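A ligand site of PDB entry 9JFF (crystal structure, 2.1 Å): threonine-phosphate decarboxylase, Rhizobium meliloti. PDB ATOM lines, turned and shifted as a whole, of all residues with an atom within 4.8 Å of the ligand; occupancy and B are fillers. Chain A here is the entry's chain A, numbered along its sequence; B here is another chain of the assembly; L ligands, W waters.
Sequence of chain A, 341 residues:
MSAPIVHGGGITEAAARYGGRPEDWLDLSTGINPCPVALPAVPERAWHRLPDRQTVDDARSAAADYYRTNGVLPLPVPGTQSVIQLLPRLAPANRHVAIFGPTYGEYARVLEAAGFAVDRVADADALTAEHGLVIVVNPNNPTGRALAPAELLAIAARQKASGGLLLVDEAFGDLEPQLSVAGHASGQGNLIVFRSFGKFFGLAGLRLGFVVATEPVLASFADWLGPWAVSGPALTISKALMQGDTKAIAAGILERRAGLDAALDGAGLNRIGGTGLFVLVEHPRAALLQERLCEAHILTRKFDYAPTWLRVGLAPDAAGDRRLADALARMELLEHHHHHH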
ATOM      1  N   ILE A   5      12.654 -21.066   6.633  1.00  0.00           N
ATOM      2  CA  ILE A   5      12.121 -20.706   5.323  1.00  0.00           C
ATOM      3  C   ILE A   5      13.169 -19.952   4.519  1.00  0.00           C
ATOM      4  O   ILE A   5      13.906 -19.111   5.049  1.00  0.00           O
ATOM      5  CB  ILE A   5      10.850 -19.850   5.507  1.00  0.00           C
ATOM      6  CG1 ILE A   5       9.725 -20.678   6.151  1.00  0.00           C
ATOM      7  CG2 ILE A   5      10.403 -19.210   4.195  1.00  0.00           C
ATOM      8  CD1 ILE A   5       8.596 -19.817   6.713  1.00  0.00           C
ATOM      9  N   HIS A   7      13.418 -17.190   2.521  1.00  0.00           N
ATOM     10  CA  HIS A   7      12.774 -15.953   2.116  1.00  0.00           C
ATOM     11  C   HIS A   7      13.520 -15.320   0.948  1.00  0.00           C
ATOM     12  O   HIS A   7      14.677 -15.652   0.662  1.00  0.00           O
ATOM     13  CB  HIS A   7      12.731 -14.967   3.290  1.00  0.00           C
ATOM     14  CG  HIS A   7      11.946 -15.461   4.467  1.00  0.00           C
ATOM     15  ND1 HIS A   7      10.577 -15.570   4.447  1.00  0.00           N
ATOM     16  CD2 HIS A   7      12.344 -15.866   5.691  1.00  0.00           C
ATOM     17  CE1 HIS A   7      10.157 -16.027   5.613  1.00  0.00           C
ATOM     18  NE2 HIS A   7      11.210 -16.212   6.387  1.00  0.00           N
ATOM     19  N   GLY A   8      12.850 -14.392   0.279  1.00  0.00           N
ATOM     20  CA  GLY A   8      13.541 -13.567  -0.702  1.00  0.00           C
ATOM     21  C   GLY A   8      14.667 -12.765  -0.083  1.00  0.00           C
ATOM     22  O   GLY A   8      14.748 -12.612   1.141  1.00  0.00           O
ATOM     23  N   SER A  29      13.784 -10.478  -5.787  1.00  0.00           N
ATOM     24  CA  SER A  29      13.165 -11.532  -4.993  1.00  0.00           C
ATOM     25  C   SER A  29      12.480 -11.005  -3.738  1.00  0.00           C
ATOM     26  O   SER A  29      11.992 -11.815  -2.932  1.00  0.00           O
ATOM     27  CB  SER A  29      14.192 -12.595  -4.617  1.00  0.00           C
ATOM     28  OG  SER A  29      15.174 -12.063  -3.739  1.00  0.00           O
ATOM     29  N   THR A  30      12.416  -9.692  -3.536  1.00  0.00           N
ATOM     30  CA  THR A  30      11.677  -9.139  -2.407  1.00  0.00           C
ATOM     31  C   THR A  30      10.604  -8.173  -2.920  1.00  0.00           C
ATOM     32  O   THR A  30      10.388  -8.040  -4.131  1.00  0.00           O
ATOM     33  CB  THR A  30      12.605  -8.418  -1.412  1.00  0.00           C
ATOM     34  OG1 THR A  30      13.058  -7.176  -1.971  1.00  0.00           O
ATOM     35  CG2 THR A  30      13.793  -9.303  -1.036  1.00  0.00           C
ATOM     36  N   GLY A  79      10.852  -4.540  13.746  1.00  0.00           N
ATOM     37  CA  GLY A  79      10.423  -5.405  12.657  1.00  0.00           C
ATOM     38  C   GLY A  79       9.181  -6.181  13.045  1.00  0.00           C
ATOM     39  O   GLY A  79       9.076  -6.644  14.186  1.00  0.00           O
ATOM     40  N   THR A  80       8.215  -6.305  12.124  1.00  0.00           N
ATOM     41  CA  THR A  80       7.021  -7.058  12.470  1.00  0.00           C
ATOM     42  C   THR A  80       7.328  -8.535  12.697  1.00  0.00           C
ATOM     43  O   THR A  80       6.580  -9.209  13.402  1.00  0.00           O
ATOM     44  CB  THR A  80       5.920  -6.901  11.403  1.00  0.00           C
ATOM     45  OG1 THR A  80       6.417  -7.296  10.119  1.00  0.00           O
ATOM     46  CG2 THR A  80       5.478  -5.447  11.322  1.00  0.00           C
ATOM     47  N   GLN A  81       8.433  -9.027  12.139  1.00  0.00           N
ATOM     48  CA  GLN A  81       8.864 -10.380  12.458  1.00  0.00           C
ATOM     49  C   GLN A  81       8.964 -10.590  13.964  1.00  0.00           C
ATOM     50  O   GLN A  81       8.632 -11.658  14.476  1.00  0.00           O
ATOM     51  CB  GLN A  81      10.206 -10.684  11.782  1.00  0.00           C
ATOM     52  CG  GLN A  81      10.563 -12.167  11.834  1.00  0.00           C
ATOM     53  CD  GLN A  81       9.500 -13.032  11.159  1.00  0.00           C
ATOM     54  OE1 GLN A  81       8.986 -12.677  10.100  1.00  0.00           O
ATOM     55  NE2 GLN A  81       9.170 -14.148  11.792  1.00  0.00           N
ATOM     56  N   ILE A  84       5.513 -11.190  15.207  1.00  0.00           N
ATOM     57  CA  ILE A  84       5.053 -12.492  14.728  1.00  0.00           C
ATOM     58  C   ILE A  84       5.577 -13.597  15.653  1.00  0.00           C
ATOM     59  O   ILE A  84       4.804 -14.447  16.114  1.00  0.00           O
ATOM     60  CB  ILE A  84       5.473 -12.730  13.267  1.00  0.00           C
ATOM     61  CG1 ILE A  84       4.791 -11.724  12.341  1.00  0.00           C
ATOM     62  CG2 ILE A  84       5.105 -14.143  12.837  1.00  0.00           C
ATOM     63  CD1 ILE A  84       5.263 -11.817  10.886  1.00  0.00           C
ATOM     64  N   TYR A 104       2.543 -15.269   3.520  1.00  0.00           N
ATOM     65  CA  TYR A 104       3.826 -15.221   4.219  1.00  0.00           C
ATOM     66  C   TYR A 104       3.914 -16.372   5.216  1.00  0.00           C
ATOM     67  O   TYR A 104       3.006 -16.600   6.017  1.00  0.00           O
ATOM     68  CB  TYR A 104       3.954 -13.862   4.917  1.00  0.00           C
ATOM     69  CG  TYR A 104       5.299 -13.607   5.537  1.00  0.00           C
ATOM     70  CD1 TYR A 104       6.457 -13.596   4.761  1.00  0.00           C
ATOM     71  CD2 TYR A 104       5.409 -13.335   6.896  1.00  0.00           C
ATOM     72  CE1 TYR A 104       7.694 -13.352   5.337  1.00  0.00           C
ATOM     73  CE2 TYR A 104       6.632 -13.076   7.480  1.00  0.00           C
ATOM     74  CZ  TYR A 104       7.778 -13.091   6.693  1.00  0.00           C
ATOM     75  OH  TYR A 104       8.992 -12.833   7.289  1.00  0.00           O
ATOM     76  N   TYR A 107       3.939 -17.011   9.822  1.00  0.00           N
ATOM     77  CA  TYR A 107       2.789 -17.151  10.725  1.00  0.00           C
ATOM     78  C   TYR A 107       2.539 -18.619  11.071  1.00  0.00           C
ATOM     79  O   TYR A 107       2.465 -18.984  12.252  1.00  0.00           O
ATOM     80  CB  TYR A 107       1.551 -16.524  10.097  1.00  0.00           C
ATOM     81  CG  TYR A 107       1.618 -15.023  10.068  1.00  0.00           C
ATOM     82  CD1 TYR A 107       1.474 -14.302  11.252  1.00  0.00           C
ATOM     83  CD2 TYR A 107       1.846 -14.322   8.895  1.00  0.00           C
ATOM     84  CE1 TYR A 107       1.550 -12.916  11.264  1.00  0.00           C
ATOM     85  CE2 TYR A 107       1.914 -12.932   8.884  1.00  0.00           C
ATOM     86  CZ  TYR A 107       1.775 -12.241  10.069  1.00  0.00           C
ATOM     87  OH  TYR A 107       1.838 -10.863  10.097  1.00  0.00           O
ATOM     88  N   VAL A 137      -3.169 -11.256   5.674  1.00  0.00           N
ATOM     89  CA  VAL A 137      -2.191 -10.341   5.121  1.00  0.00           C
ATOM     90  C   VAL A 137      -2.893  -9.536   4.023  1.00  0.00           C
ATOM     91  O   VAL A 137      -3.370 -10.103   3.038  1.00  0.00           O
ATOM     92  CB  VAL A 137      -0.965 -11.093   4.579  1.00  0.00           C
ATOM     93  CG1 VAL A 137       0.027 -10.125   3.953  1.00  0.00           C
ATOM     94  CG2 VAL A 137      -0.299 -11.890   5.695  1.00  0.00           C
ATOM     95  N   ASN A 141       0.648 -11.110   0.523  1.00  0.00           N
ATOM     96  CA  ASN A 141       1.915 -11.572  -0.010  1.00  0.00           C
ATOM     97  C   ASN A 141       1.794 -13.083  -0.117  1.00  0.00           C
ATOM     98  O   ASN A 141       1.592 -13.741   0.910  1.00  0.00           O
ATOM     99  CB  ASN A 141       3.049 -11.167   0.934  1.00  0.00           C
ATOM    100  CG  ASN A 141       4.380 -11.852   0.632  1.00  0.00           C
ATOM    101  OD1 ASN A 141       4.526 -12.583  -0.350  1.00  0.00           O
ATOM    102  ND2 ASN A 141       5.373 -11.620   1.493  1.00  0.00           N
ATOM    103  N   ASP A 169      -2.265  -7.976   8.706  1.00  0.00           N
ATOM    104  CA  ASP A 169      -0.897  -7.573   8.415  1.00  0.00           C
ATOM    105  C   ASP A 169      -0.920  -6.710   7.152  1.00  0.00           C
ATOM    106  O   ASP A 169      -1.083  -7.224   6.041  1.00  0.00           O
ATOM    107  CB  ASP A 169      -0.013  -8.804   8.259  1.00  0.00           C
ATOM    108  CG  ASP A 169       1.438  -8.467   7.971  1.00  0.00           C
ATOM    109  OD1 ASP A 169       1.767  -7.306   7.649  1.00  0.00           O
ATOM    110  OD2 ASP A 169       2.257  -9.404   8.046  1.00  0.00           O
ATOM    111  N   ALA A 171       1.571  -4.947   5.855  1.00  0.00           N
ATOM    112  CA  ALA A 171       2.961  -4.649   5.483  1.00  0.00           C
ATOM    113  C   ALA A 171       3.047  -3.976   4.117  1.00  0.00           C
ATOM    114  O   ALA A 171       3.877  -3.092   3.902  1.00  0.00           O
ATOM    115  CB  ALA A 171       3.786  -5.937   5.499  1.00  0.00           C
ATOM    116  N   PHE A 172       2.196  -4.389   3.177  1.00  0.00           N
ATOM    117  CA  PHE A 172       2.228  -3.878   1.820  1.00  0.00           C
ATOM    118  C   PHE A 172       1.075  -2.929   1.518  1.00  0.00           C
ATOM    119  O   PHE A 172       0.654  -2.785   0.369  1.00  0.00           O
ATOM    120  CB  PHE A 172       2.251  -5.048   0.827  1.00  0.00           C
ATOM    121  CG  PHE A 172       3.558  -5.791   0.819  1.00  0.00           C
ATOM    122  CD1 PHE A 172       4.652  -5.271   0.143  1.00  0.00           C
ATOM    123  CD2 PHE A 172       3.701  -6.984   1.501  1.00  0.00           C
ATOM    124  CE1 PHE A 172       5.859  -5.947   0.138  1.00  0.00           C
ATOM    125  CE2 PHE A 172       4.903  -7.668   1.500  1.00  0.00           C
ATOM    126  CZ  PHE A 172       5.989  -7.146   0.819  1.00  0.00           C
ATOM    127  N   SER A 196       4.609  -2.442   8.551  1.00  0.00           N
ATOM    128  CA  SER A 196       6.035  -2.625   8.334  1.00  0.00           C
ATOM    129  C   SER A 196       6.618  -1.363   7.705  1.00  0.00           C
ATOM    130  O   SER A 196       6.015  -0.752   6.813  1.00  0.00           O
ATOM    131  CB  SER A 196       6.312  -3.845   7.443  1.00  0.00           C
ATOM    132  OG  SER A 196       7.674  -3.901   7.058  1.00  0.00           O
ATOM    133  N   LYS A 199       9.413  -1.934   3.662  1.00  0.00           N
ATOM    134  CA  LYS A 199       9.045  -2.175   2.274  1.00  0.00           C
ATOM    135  C   LYS A 199       8.758  -0.871   1.529  1.00  0.00           C
ATOM    136  O   LYS A 199       9.364  -0.596   0.485  1.00  0.00           O
ATOM    137  CB  LYS A 199       7.845  -3.111   2.187  1.00  0.00           C
ATOM    138  CG  LYS A 199       8.208  -4.568   2.483  1.00  0.00           C
ATOM    139  CD  LYS A 199       7.471  -5.072   3.694  1.00  0.00           C
ATOM    140  CE  LYS A 199       7.942  -6.473   4.064  1.00  0.00           C
ATOM    141  NZ  LYS A 199       9.442  -6.579   4.135  1.00  0.00           N
ATOM    142  N   ARG A 207      15.286  -2.322  11.178  1.00  0.00           N
ATOM    143  CA  ARG A 207      14.301  -3.307  11.631  1.00  0.00           C
ATOM    144  C   ARG A 207      13.240  -2.539  12.419  1.00  0.00           C
ATOM    145  O   ARG A 207      13.424  -2.225  13.599  1.00  0.00           O
ATOM    146  CB  ARG A 207      14.988  -4.392  12.458  1.00  0.00           C
ATOM    147  CG  ARG A 207      16.184  -5.002  11.720  1.00  0.00           C
ATOM    148  CD  ARG A 207      15.793  -5.618  10.355  1.00  0.00           C
ATOM    149  NE  ARG A 207      14.760  -6.644  10.498  1.00  0.00           N
ATOM    150  CZ  ARG A 207      13.579  -6.622   9.888  1.00  0.00           C
ATOM    151  NH1 ARG A 207      13.274  -5.701   8.985  1.00  0.00           N
ATOM    152  NH2 ARG A 207      12.689  -7.564  10.187  1.00  0.00           N
ATOM    153  N   LEU A 208      12.136  -2.205  11.742  1.00  0.00           N
ATOM    154  CA  LEU A 208      11.098  -1.384  12.358  1.00  0.00           C
ATOM    155  C   LEU A 208       9.721  -1.702  11.797  1.00  0.00           C
ATOM    156  O   LEU A 208       9.531  -1.751  10.582  1.00  0.00           O
ATOM    157  CB  LEU A 208      11.394   0.106  12.162  1.00  0.00           C
ATOM    158  CG  LEU A 208      10.316   1.055  12.680  1.00  0.00           C
ATOM    159  CD1 LEU A 208      10.171   0.975  14.202  1.00  0.00           C
ATOM    160  CD2 LEU A 208      10.618   2.474  12.245  1.00  0.00           C
ATOM    161  N   ARG A 301      11.738 -14.826  -6.688  1.00  0.00           N
ATOM    162  CA  ARG A 301      11.200 -15.632  -5.602  1.00  0.00           C
ATOM    163  C   ARG A 301      10.325 -16.750  -6.160  1.00  0.00           C
ATOM    164  O   ARG A 301       9.313 -16.471  -6.826  1.00  0.00           O
ATOM    165  CB  ARG A 301      10.396 -14.759  -4.635  1.00  0.00           C
ATOM    166  CG  ARG A 301       9.760 -15.521  -3.450  1.00  0.00           C
ATOM    167  CD  ARG A 301      10.787 -16.031  -2.422  1.00  0.00           C
ATOM    168  NE  ARG A 301      10.226 -16.135  -1.076  1.00  0.00           N
ATOM    169  CZ  ARG A 301       9.730 -17.241  -0.538  1.00  0.00           C
ATOM    170  NH1 ARG A 301       9.733 -18.396  -1.202  1.00  0.00           N
ATOM    171  NH2 ARG A 301       9.197 -17.190   0.675  1.00  0.00           N
ATOM    172  N   ARG A 311       7.346 -14.757  -7.995  1.00  0.00           N
ATOM    173  CA  ARG A 311       7.136 -13.390  -7.536  1.00  0.00           C
ATOM    174  C   ARG A 311       8.343 -12.552  -7.926  1.00  0.00           C
ATOM    175  O   ARG A 311       9.488 -12.906  -7.608  1.00  0.00           O
ATOM    176  CB  ARG A 311       6.924 -13.319  -6.015  1.00  0.00           C
ATOM    177  CG  ARG A 311       6.405 -11.956  -5.563  1.00  0.00           C
ATOM    178  CD  ARG A 311       6.453 -11.803  -4.048  1.00  0.00           C
ATOM    179  NE  ARG A 311       7.821 -11.895  -3.528  1.00  0.00           N
ATOM    180  CZ  ARG A 311       8.116 -12.331  -2.310  1.00  0.00           C
ATOM    181  NH1 ARG A 311       7.190 -12.736  -1.467  1.00  0.00           N
ATOM    182  NH2 ARG A 311       9.400 -12.363  -1.933  1.00  0.00           N
ATOM    183  N   LEU B  50      17.290  -5.905   3.327  1.00  0.00           N
ATOM    184  CA  LEU B  50      17.203  -6.796   4.473  1.00  0.00           C
ATOM    185  C   LEU B  50      18.597  -7.357   4.764  1.00  0.00           C
ATOM    186  O   LEU B  50      19.338  -7.687   3.821  1.00  0.00           O
ATOM    187  CB  LEU B  50      16.218  -7.931   4.185  1.00  0.00           C
ATOM    188  CG  LEU B  50      14.734  -7.552   4.157  1.00  0.00           C
ATOM    189  CD1 LEU B  50      13.907  -8.684   3.562  1.00  0.00           C
ATOM    190  CD2 LEU B  50      14.241  -7.191   5.565  1.00  0.00           C
ATOM    191  N   TRP B 228      16.373 -11.867  10.240  1.00  0.00           N
ATOM    192  CA  TRP B 228      16.656 -10.428  10.188  1.00  0.00           C
ATOM    193  C   TRP B 228      16.538  -9.768  11.561  1.00  0.00           C
ATOM    194  O   TRP B 228      16.032  -8.651  11.695  1.00  0.00           O
ATOM    195  CB  TRP B 228      15.736  -9.708   9.177  1.00  0.00           C
ATOM    196  CG  TRP B 228      15.517 -10.444   7.867  1.00  0.00           C
ATOM    197  CD1 TRP B 228      16.451 -10.697   6.905  1.00  0.00           C
ATOM    198  CD2 TRP B 228      14.281 -10.992   7.390  1.00  0.00           C
ATOM    199  NE1 TRP B 228      15.879 -11.389   5.857  1.00  0.00           N
ATOM    200  CE2 TRP B 228      14.550 -11.576   6.124  1.00  0.00           C
ATOM    201  CE3 TRP B 228      12.980 -11.061   7.897  1.00  0.00           C
ATOM    202  CZ2 TRP B 228      13.564 -12.214   5.375  1.00  0.00           C
ATOM    203  CZ3 TRP B 228      11.998 -11.692   7.144  1.00  0.00           C
ATOM    204  CH2 TRP B 228      12.298 -12.260   5.893  1.00  0.00           C
HETATM  205  N1  LIG L   1       4.574  -9.425   6.861  1.00  0.00           N
HETATM  206  C1  LIG L   1       4.713  -9.748   5.575  1.00  0.00           C
HETATM  207  C2  LIG L   1       3.486 -10.021   4.766  1.00  0.00           C
HETATM  208  C3  LIG L   1       5.986  -9.843   4.988  1.00  0.00           C
HETATM  209  O1  LIG L   1       6.083 -10.185   3.669  1.00  0.00           O
HETATM  210  C4  LIG L   1       7.120  -9.600   5.778  1.00  0.00           C
HETATM  211  C5  LIG L   1       8.506  -9.672   5.198  1.00  0.00           C
HETATM  212  C6  LIG L   1       6.946  -9.247   7.121  1.00  0.00           C
HETATM  213  C7  LIG L   1       5.655  -9.177   7.604  1.00  0.00           C
HETATM  214  C8  LIG L   1       8.117  -8.966   8.011  1.00  0.00           C
HETATM  215  O2  LIG L   1       8.697  -7.679   7.638  1.00  0.00           O
HETATM  216  P1  LIG L   1       9.436  -6.720   8.706  1.00  0.00           P
HETATM  217  O3  LIG L   1       8.372  -5.746   9.193  1.00  0.00           O
HETATM  218  O4  LIG L   1      10.546  -6.043   7.933  1.00  0.00           O
HETATM  219  O5  LIG L   1       9.936  -7.648   9.805  1.00  0.00           O
HETATM  220  P2  LIG L   1       9.167 -13.727   1.596  1.00  0.00           P
HETATM  221  O6  LIG L   1       9.069 -15.015   2.394  1.00  0.00           O
HETATM  222  O7  LIG L   1      10.083 -13.839   0.387  1.00  0.00           O
HETATM  223  O8  LIG L   1       7.803 -13.153   1.250  1.00  0.00           O
HETATM  224  N2  LIG L   1       8.624 -10.450   3.981  1.00  0.00           N
HETATM  225  C9  LIG L   1       9.986 -10.385   3.421  1.00  0.00           C
HETATM  226  C10 LIG L   1      10.102 -11.262   2.195  1.00  0.00           C
HETATM  227  O9  LIG L   1       9.844 -12.651   2.594  1.00  0.00           O
HETATM  228  C11 LIG L   1      11.486 -11.197   1.571  1.00  0.00           C
HETATM  229  O   HOH W   1      11.130  -8.297   6.198  1.00  0.00           O
HETATM  230  O   HOH W   2       7.404 -16.772   3.621  1.00  0.00           O
HETATM  231  O   HOH W   3      10.430  -3.391   8.347  1.00  0.00           O
HETATM  232  O   HOH W   4       5.731 -14.920   0.878  1.00  0.00           O
HETATM  233  O   HOH W   5      11.369  -4.779   5.626  1.00  0.00           O
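Residues that only touch the ligand: Tyr 104, Phe 172, Val 137, Gly 79, Ala 171, Trp 228 of chain B and Thr 30. Hydrophobic or aromatic side chains that line the ligand: His 7, Tyr 104, Val 137, Ala 171, Phe 172 and Trp 228 of chain B. Within 4 Å of the ligand: His 7, Gly 8, Thr 30, Gly 79, Thr 80, Gln 81, Tyr 104, Val 137, Asn 141, Asp 169, Ala 171, Phe 172, Ser 196, Lys 199, Arg 207, Arg 301, Arg 311 and Trp 228 of chain B.
Water W3 lies within hydrogen-bond range of O4 of the ligand (2.7 Å), O of Leu 208 (2.9 Å) and OG of Ser 196 (3.1 Å). Water W2 lies within hydrogen-bond range of O6 of the ligand (2.7 Å), NH2 of Arg 301 (3.5 Å) and ND1 of His 7 (3.5 Å). Water W4 bridges O8 of the ligand (2.7 Å) and OD1 of Asn 141 (2.9 Å). Water W5 bridges O4 of the ligand (2.8 Å) and NZ of Lys 199 (3.0 Å). Water W1 bridges O2 of the ligand (2.9 Å) and NZ of Lys 199 (3.2 Å).
OD2 of Asp 169 sits at hydrogen-bond distance from N1 of the ligand, 2.6 Å away. An oxygen (O6) of the ligand sits at hydrogen-bond distance from a ring nitrogen (ND1) of His 7, 2.6 Å away. An oxygen (O3) of the ligand sits at hydrogen-bond distance from the backbone NH of Thr 80 (3.0 Å). OG1 of Thr 80 sits at hydrogen-bond distance from O3 of the ligand, at 2.7 Å. An oxygen (O1) of the ligand lies within hydrogen-bond range of the side-chain amide nitrogen (ND2) of Asn 141 (2.7 Å). The guanidinium group (NE) of Arg 301 is in salt-bridge range of an oxygen (O7) of the ligand (2.7 Å). NH2 of Arg 207 is in salt-bridge range of O5 of the ligand. NH1 of Arg 311 is in salt-bridge range of O8 of the ligand, 2.8 Å away. The backbone NH (N) of Gly 8 is in hydrogen-bond range of an oxygen (O7) of the ligand (2.8 Å). The side-chain hydroxyl (OG) of Ser 196 lies within hydrogen-bond range of an oxygen (O3) of the ligand, 2.9 Å away. An oxygen (O5) of the ligand is in hydrogen-bond range of the backbone NH of Gln 81 (3.1 Å). An oxygen (O4) of the ligand lies within salt-bridge range of the side-chain amino group (NZ) of Lys 199 (3.99 Å).
The side-chain carboxylate (OD1) of Asp 169 sits at hydrogen-bond distance from the backbone NH (N) of Ala 171 (3.0 Å). The side-chain hydroxyl (OH) of Tyr 107 lies within hydrogen-bond range of the side-chain carboxylate (OD2) of Asp 169. The guanidinium group of Arg 311 lies within hydrogen-bond range of the side-chain amide oxygen of Asn 141 (2.9 Å). The backbone carbonyl oxygen (O) of Asn 141 sits at hydrogen-bond distance from the backbone NH (N) of Tyr 104, at 3.2 Å. The backbone NH of Arg 311 is in hydrogen-bond range of the backbone carbonyl oxygen of Arg 301 (2.9 Å). O of Arg 207 lies close to N of Gly 79 (3.5 Å). The guanidinium group of Arg 207 is in hydrogen-bond range of the backbone carbonyl oxygen of Trp 228 of chain B. The side-chain amide oxygen (OE1) of Gln 81 is in hydrogen-bond range of the side-chain hydroxyl (OH) of Tyr 104 (2.8 Å).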
